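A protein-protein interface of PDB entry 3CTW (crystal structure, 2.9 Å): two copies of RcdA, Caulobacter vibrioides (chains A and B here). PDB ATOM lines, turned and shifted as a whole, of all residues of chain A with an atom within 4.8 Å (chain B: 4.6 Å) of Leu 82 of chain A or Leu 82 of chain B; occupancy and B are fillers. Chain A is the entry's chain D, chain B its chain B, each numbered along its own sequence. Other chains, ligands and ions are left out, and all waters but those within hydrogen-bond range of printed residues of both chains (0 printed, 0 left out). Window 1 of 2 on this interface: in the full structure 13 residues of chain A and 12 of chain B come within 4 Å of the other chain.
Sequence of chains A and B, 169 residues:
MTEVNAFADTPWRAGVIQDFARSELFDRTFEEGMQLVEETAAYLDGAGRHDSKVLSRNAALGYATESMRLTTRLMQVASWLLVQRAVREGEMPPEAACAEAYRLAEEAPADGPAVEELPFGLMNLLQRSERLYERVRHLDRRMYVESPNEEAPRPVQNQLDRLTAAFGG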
ATOM      1  N   PHE A  30      -7.104   7.535  17.779  1.00  0.00           N
ATOM      2  CA  PHE A  30      -6.208   8.121  16.790  1.00  0.00           C
ATOM      3  C   PHE A  30      -4.879   7.373  16.752  1.00  0.00           C
ATOM      4  O   PHE A  30      -4.401   7.013  15.677  1.00  0.00           O
ATOM      5  CB  PHE A  30      -5.956   9.601  17.079  1.00  0.00           C
ATOM      6  CG  PHE A  30      -5.058  10.261  16.071  1.00  0.00           C
ATOM      7  CD1 PHE A  30      -5.568  10.718  14.865  1.00  0.00           C
ATOM      8  CD2 PHE A  30      -3.699  10.422  16.322  1.00  0.00           C
ATOM      9  CE1 PHE A  30      -4.739  11.329  13.938  1.00  0.00           C
ATOM     10  CE2 PHE A  30      -2.873  11.014  15.393  1.00  0.00           C
ATOM     11  CZ  PHE A  30      -3.388  11.458  14.204  1.00  0.00           C
ATOM     12  N   ALA A  78      -8.135   6.563   8.602  1.00  0.00           N
ATOM     13  CA  ALA A  78      -7.009   7.491   8.670  1.00  0.00           C
ATOM     14  C   ALA A  78      -7.417   8.895   8.193  1.00  0.00           C
ATOM     15  O   ALA A  78      -7.101   9.902   8.836  1.00  0.00           O
ATOM     16  CB  ALA A  78      -5.830   6.955   7.853  1.00  0.00           C
ATOM     17  N   SER A  79      -8.167   8.942   7.095  1.00  0.00           N
ATOM     18  CA  SER A  79      -8.661  10.199   6.552  1.00  0.00           C
ATOM     19  C   SER A  79      -9.656  10.846   7.508  1.00  0.00           C
ATOM     20  O   SER A  79      -9.623  12.049   7.701  1.00  0.00           O
ATOM     21  CB  SER A  79      -9.301   9.986   5.185  1.00  0.00           C
ATOM     22  OG  SER A  79     -10.401   9.109   5.286  1.00  0.00           O
ATOM     23  N   TRP A  80     -10.502  10.036   8.136  1.00  0.00           N
ATOM     24  CA  TRP A  80     -11.436  10.538   9.129  1.00  0.00           C
ATOM     25  C   TRP A  80     -10.700  11.090  10.351  1.00  0.00           C
ATOM     26  O   TRP A  80     -10.894  12.241  10.730  1.00  0.00           O
ATOM     27  CB  TRP A  80     -12.428   9.455   9.543  1.00  0.00           C
ATOM     28  CG  TRP A  80     -13.529   9.974  10.428  1.00  0.00           C
ATOM     29  CD1 TRP A  80     -14.748  10.423  10.027  1.00  0.00           C
ATOM     30  CD2 TRP A  80     -13.508  10.101  11.861  1.00  0.00           C
ATOM     31  NE1 TRP A  80     -15.492  10.813  11.113  1.00  0.00           N
ATOM     32  CE2 TRP A  80     -14.755  10.628  12.250  1.00  0.00           C
ATOM     33  CE3 TRP A  80     -12.561   9.809  12.850  1.00  0.00           C
ATOM     34  CZ2 TRP A  80     -15.087  10.868  13.588  1.00  0.00           C
ATOM     35  CZ3 TRP A  80     -12.889  10.059  14.188  1.00  0.00           C
ATOM     36  CH2 TRP A  80     -14.141  10.587  14.538  1.00  0.00           C
ATOM     37  N   LEU A  81      -9.804  10.285  10.910  1.00  0.00           N
ATOM     38  CA  LEU A  81      -9.053  10.674  12.093  1.00  0.00           C
ATOM     39  C   LEU A  81      -8.423  12.044  11.931  1.00  0.00           C
ATOM     40  O   LEU A  81      -8.534  12.892  12.808  1.00  0.00           O
ATOM     41  CB  LEU A  81      -7.982   9.634  12.424  1.00  0.00           C
ATOM     42  CG  LEU A  81      -8.534   8.367  13.101  1.00  0.00           C
ATOM     43  CD1 LEU A  81      -7.453   7.309  13.358  1.00  0.00           C
ATOM     44  CD2 LEU A  81      -9.197   8.768  14.393  1.00  0.00           C
ATOM     45  N   LEU A  82      -7.770  12.265  10.802  1.00  0.00           N
ATOM     46  CA  LEU A  82      -7.062  13.516  10.573  1.00  0.00           C
ATOM     47  C   LEU A  82      -7.994  14.682  10.353  1.00  0.00           C
ATOM     48  O   LEU A  82      -7.573  15.822  10.327  1.00  0.00           O
ATOM     49  CB  LEU A  82      -6.182  13.385   9.332  1.00  0.00           C
ATOM     50  CG  LEU A  82      -4.959  12.482   9.493  1.00  0.00           C
ATOM     51  CD1 LEU A  82      -4.397  12.092   8.148  1.00  0.00           C
ATOM     52  CD2 LEU A  82      -3.888  13.157  10.388  1.00  0.00           C
ATOM     53  N   VAL A  83      -9.244  14.426  10.095  1.00  0.00           N
ATOM     54  CA  VAL A  83      -9.898  15.528   9.536  1.00  0.00           C
ATOM     55  C   VAL A  83     -10.709  16.100  10.618  1.00  0.00           C
ATOM     56  O   VAL A  83     -10.799  17.296  10.769  1.00  0.00           O
ATOM     57  CB  VAL A  83     -10.870  15.068   8.408  1.00  0.00           C
ATOM     58  CG1 VAL A  83     -12.091  15.977   8.249  1.00  0.00           C
ATOM     59  CG2 VAL A  83     -10.133  14.949   7.112  1.00  0.00           C
ATOM     60  N   GLN A  84     -11.196  15.275  11.512  1.00  0.00           N
ATOM     61  CA  GLN A  84     -11.099  15.505  12.921  1.00  0.00           C
ATOM     62  C   GLN A  84      -9.938  16.165  13.495  1.00  0.00           C
ATOM     63  O   GLN A  84     -10.067  17.063  14.312  1.00  0.00           O
ATOM     64  CB  GLN A  84     -11.495  14.279  13.699  1.00  0.00           C
ATOM     65  CG  GLN A  84     -12.582  13.538  12.998  1.00  0.00           C
ATOM     66  CD  GLN A  84     -13.858  14.355  12.854  1.00  0.00           C
ATOM     67  OE1 GLN A  84     -14.633  14.160  11.923  1.00  0.00           O
ATOM     68  NE2 GLN A  84     -14.049  15.306  13.747  1.00  0.00           N
ATOM     69  N   ARG A  85      -8.785  15.717  13.088  1.00  0.00           N
ATOM     70  CA  ARG A  85      -7.597  16.257  13.741  1.00  0.00           C
ATOM     71  C   ARG A  85      -7.402  17.718  13.354  1.00  0.00           C
ATOM     72  O   ARG A  85      -7.132  18.563  14.201  1.00  0.00           O
ATOM     73  CB  ARG A  85      -6.370  15.443  13.375  1.00  0.00           C
ATOM     74  CG  ARG A  85      -5.145  15.749  14.242  1.00  0.00           C
ATOM     75  CD  ARG A  85      -4.231  14.544  14.249  1.00  0.00           C
ATOM     76  NE  ARG A  85      -3.304  14.544  13.115  1.00  0.00           N
ATOM     77  CZ  ARG A  85      -2.128  15.141  13.150  1.00  0.00           C
ATOM     78  NH1 ARG A  85      -1.769  15.798  14.242  1.00  0.00           N
ATOM     79  NH2 ARG A  85      -1.329  15.095  12.090  1.00  0.00           N
ATOM     80  N   ALA A  86      -7.570  18.012  12.069  1.00  0.00           N
ATOM     81  CA  ALA A  86      -7.454  19.371  11.569  1.00  0.00           C
ATOM     82  C   ALA A  86      -8.567  20.257  12.110  1.00  0.00           C
ATOM     83  O   ALA A  86      -8.336  21.416  12.433  1.00  0.00           O
ATOM     84  CB  ALA A  86      -7.474  19.372  10.066  1.00  0.00           C
ATOM     85  N   MET A  92      -9.359  23.109   9.785  1.00  0.00           N
ATOM     86  CA  MET A  92     -10.607  22.997   9.051  1.00  0.00           C
ATOM     87  C   MET A  92     -11.756  23.374   9.967  1.00  0.00           C
ATOM     88  O   MET A  92     -11.749  23.043  11.152  1.00  0.00           O
ATOM     89  CB  MET A  92     -10.818  21.573   8.532  1.00  0.00           C
ATOM     90  CG  MET A  92      -9.852  21.123   7.474  1.00  0.00           C
ATOM     91  SD  MET A  92     -10.723  20.215   6.203  1.00  0.00           S
ATOM     92  CE  MET A  92     -10.978  18.697   7.052  1.00  0.00           C
ATOM     93  N   PHE B  30      -1.716  22.814  -0.767  1.00  0.00           N
ATOM     94  CA  PHE B  30      -2.315  22.581   0.553  1.00  0.00           C
ATOM     95  C   PHE B  30      -3.064  23.816   1.043  1.00  0.00           C
ATOM     96  O   PHE B  30      -4.144  23.709   1.635  1.00  0.00           O
ATOM     97  CB  PHE B  30      -1.246  22.203   1.582  1.00  0.00           C
ATOM     98  CG  PHE B  30      -1.807  21.869   2.943  1.00  0.00           C
ATOM     99  CD1 PHE B  30      -2.263  20.595   3.216  1.00  0.00           C
ATOM    100  CD2 PHE B  30      -1.876  22.822   3.950  1.00  0.00           C
ATOM    101  CE1 PHE B  30      -2.784  20.271   4.456  1.00  0.00           C
ATOM    102  CE2 PHE B  30      -2.399  22.499   5.190  1.00  0.00           C
ATOM    103  CZ  PHE B  30      -2.857  21.224   5.438  1.00  0.00           C
ATOM    104  N   ALA B  78      -9.182  17.473   0.643  1.00  0.00           N
ATOM    105  CA  ALA B  78      -8.801  17.617   2.037  1.00  0.00           C
ATOM    106  C   ALA B  78      -8.162  16.336   2.581  1.00  0.00           C
ATOM    107  O   ALA B  78      -7.095  16.378   3.191  1.00  0.00           O
ATOM    108  CB  ALA B  78     -10.002  18.006   2.859  1.00  0.00           C
ATOM    109  N   SER B  79      -8.801  15.196   2.315  1.00  0.00           N
ATOM    110  CA  SER B  79      -8.307  13.894   2.743  1.00  0.00           C
ATOM    111  C   SER B  79      -6.957  13.562   2.113  1.00  0.00           C
ATOM    112  O   SER B  79      -6.090  12.976   2.762  1.00  0.00           O
ATOM    113  CB  SER B  79      -9.322  12.802   2.401  1.00  0.00           C
ATOM    114  OG  SER B  79     -10.579  13.058   2.993  1.00  0.00           O
ATOM    115  N   TRP B  80      -6.780  13.962   0.859  1.00  0.00           N
ATOM    116  CA  TRP B  80      -5.562  13.676   0.130  1.00  0.00           C
ATOM    117  C   TRP B  80      -4.399  14.486   0.712  1.00  0.00           C
ATOM    118  O   TRP B  80      -3.338  13.941   1.021  1.00  0.00           O
ATOM    119  CB  TRP B  80      -5.766  13.984  -1.357  1.00  0.00           C
ATOM    120  CG  TRP B  80      -4.662  13.453  -2.210  1.00  0.00           C
ATOM    121  CD1 TRP B  80      -4.616  12.240  -2.811  1.00  0.00           C
ATOM    122  CD2 TRP B  80      -3.427  14.113  -2.540  1.00  0.00           C
ATOM    123  NE1 TRP B  80      -3.438  12.098  -3.501  1.00  0.00           N
ATOM    124  CE2 TRP B  80      -2.690  13.234  -3.348  1.00  0.00           C
ATOM    125  CE3 TRP B  80      -2.880  15.362  -2.230  1.00  0.00           C
ATOM    126  CZ2 TRP B  80      -1.431  13.563  -3.856  1.00  0.00           C
ATOM    127  CZ3 TRP B  80      -1.629  15.690  -2.736  1.00  0.00           C
ATOM    128  CH2 TRP B  80      -0.920  14.795  -3.541  1.00  0.00           C
ATOM    129  N   LEU B  81      -4.637  15.785   0.875  1.00  0.00           N
ATOM    130  CA  LEU B  81      -3.644  16.733   1.361  1.00  0.00           C
ATOM    131  C   LEU B  81      -3.208  16.455   2.793  1.00  0.00           C
ATOM    132  O   LEU B  81      -2.045  16.640   3.136  1.00  0.00           O
ATOM    133  CB  LEU B  81      -4.223  18.143   1.298  1.00  0.00           C
ATOM    134  CG  LEU B  81      -4.078  19.058   0.082  1.00  0.00           C
ATOM    135  CD1 LEU B  81      -4.385  18.335  -1.188  1.00  0.00           C
ATOM    136  CD2 LEU B  81      -5.053  20.223   0.255  1.00  0.00           C
ATOM    137  N   LEU B  82      -4.143  16.018   3.633  1.00  0.00           N
ATOM    138  CA  LEU B  82      -3.843  15.745   5.035  1.00  0.00           C
ATOM    139  C   LEU B  82      -3.060  14.441   5.213  1.00  0.00           C
ATOM    140  O   LEU B  82      -2.188  14.352   6.081  1.00  0.00           O
ATOM    141  CB  LEU B  82      -5.125  15.731   5.873  1.00  0.00           C
ATOM    142  CG  LEU B  82      -5.848  17.058   6.074  1.00  0.00           C
ATOM    143  CD1 LEU B  82      -7.236  16.755   6.537  1.00  0.00           C
ATOM    144  CD2 LEU B  82      -5.129  17.964   7.062  1.00  0.00           C
ATOM    145  N   VAL B  83      -3.362  13.453   4.372  1.00  0.00           N
ATOM    146  CA  VAL B  83      -2.641  12.183   4.379  1.00  0.00           C
ATOM    147  C   VAL B  83      -1.207  12.373   3.895  1.00  0.00           C
ATOM    148  O   VAL B  83      -0.263  11.897   4.523  1.00  0.00           O
ATOM    149  CB  VAL B  83      -3.357  11.101   3.532  1.00  0.00           C
ATOM    150  CG1 VAL B  83      -2.446   9.918   3.284  1.00  0.00           C
ATOM    151  CG2 VAL B  83      -4.621  10.637   4.227  1.00  0.00           C
ATOM    152  N   GLN B  84      -1.052  13.122   2.812  1.00  0.00           N
ATOM    153  CA  GLN B  84       0.259  13.413   2.271  1.00  0.00           C
ATOM    154  C   GLN B  84       1.084  14.259   3.230  1.00  0.00           C
ATOM    155  O   GLN B  84       2.311  14.154   3.242  1.00  0.00           O
ATOM    156  CB  GLN B  84       0.141  14.095   0.909  1.00  0.00           C
ATOM    157  CG  GLN B  84      -0.502  13.246  -0.183  1.00  0.00           C
ATOM    158  CD  GLN B  84       0.258  11.962  -0.457  1.00  0.00           C
ATOM    159  OE1 GLN B  84      -0.335  10.889  -0.562  1.00  0.00           O
ATOM    160  NE2 GLN B  84       1.574  12.062  -0.569  1.00  0.00           N
ATOM    161  N   ARG B  85       0.415  15.079   4.044  1.00  0.00           N
ATOM    162  CA  ARG B  85       1.100  15.840   5.089  1.00  0.00           C
ATOM    163  C   ARG B  85       1.505  14.912   6.235  1.00  0.00           C
ATOM    164  O   ARG B  85       2.597  15.047   6.789  1.00  0.00           O
ATOM    165  CB  ARG B  85       0.237  16.996   5.617  1.00  0.00           C
ATOM    166  CG  ARG B  85       1.014  17.946   6.532  1.00  0.00           C
ATOM    167  CD  ARG B  85       0.158  19.004   7.160  1.00  0.00           C
ATOM    168  NE  ARG B  85      -0.847  18.444   8.047  1.00  0.00           N
ATOM    169  CZ  ARG B  85      -1.742  19.173   8.703  1.00  0.00           C
ATOM    170  NH1 ARG B  85      -1.734  20.489   8.571  1.00  0.00           N
ATOM    171  NH2 ARG B  85      -2.641  18.593   9.491  1.00  0.00           N
ATOM    172  N   ALA B  86       0.627  13.965   6.565  1.00  0.00           N
ATOM    173  CA  ALA B  86       0.896  12.991   7.625  1.00  0.00           C
ATOM    174  C   ALA B  86       2.079  12.102   7.251  1.00  0.00           C
ATOM    175  O   ALA B  86       2.859  11.698   8.106  1.00  0.00           O
ATOM    176  CB  ALA B  86      -0.352  12.141   7.910  1.00  0.00           C
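Among the printed residues, merely in contact across the chains: Ser 79 of chain A with Ser 79 of chain B, Leu 82 of chain A with Leu 82 of chain B and Val 83 of chain A with Leu 82 of chain B.
Leu 82 of chain A touches just one residue of chain B: Leu 82. Of chain A, only Leu 82 (3.8 Å) and Val 83 (3.5 Å) come within 4 Å of Leu 82 of chain B. Of the printed residues of chain B, Ser 79 of chain A touches Ser 79. Of the printed residues of chain A, Ser 79 of chain B touches Ser 79 (3.96 Å). The nearest residue of chain A that does not touch Leu 82 of chain B is Ala 86 of chain A (4.1 Å). The nearest printed residue of chain B that does not touch Val 83 of chain A is Ser 79 of chain B (4.6 Å).
Hydrophobic or aromatic side chains of chain B within 4 Å of the printed part of chain A: Leu 82. Along chain A the printed residues that touch a printed residue of chain B span positions 79 to 83. Among the printed residues, 3 pairs touch across the chains.
Ser 79 of chain A touches its own counterpart, Ser 79 of chain B. Leu 82 of chain A touches its own counterpart, Leu 82 of chain B. Val 83 of chain A touches Leu 82 of chain B, but with the chains exchanged Leu 82 of chain A does not touch Val 83 of chain B (4.1 Å). 10 positions are printed for both chains. Of the 3 pairs that touch across the chains among the printed residues, 2 have their exchanged pair printed and touching as well.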
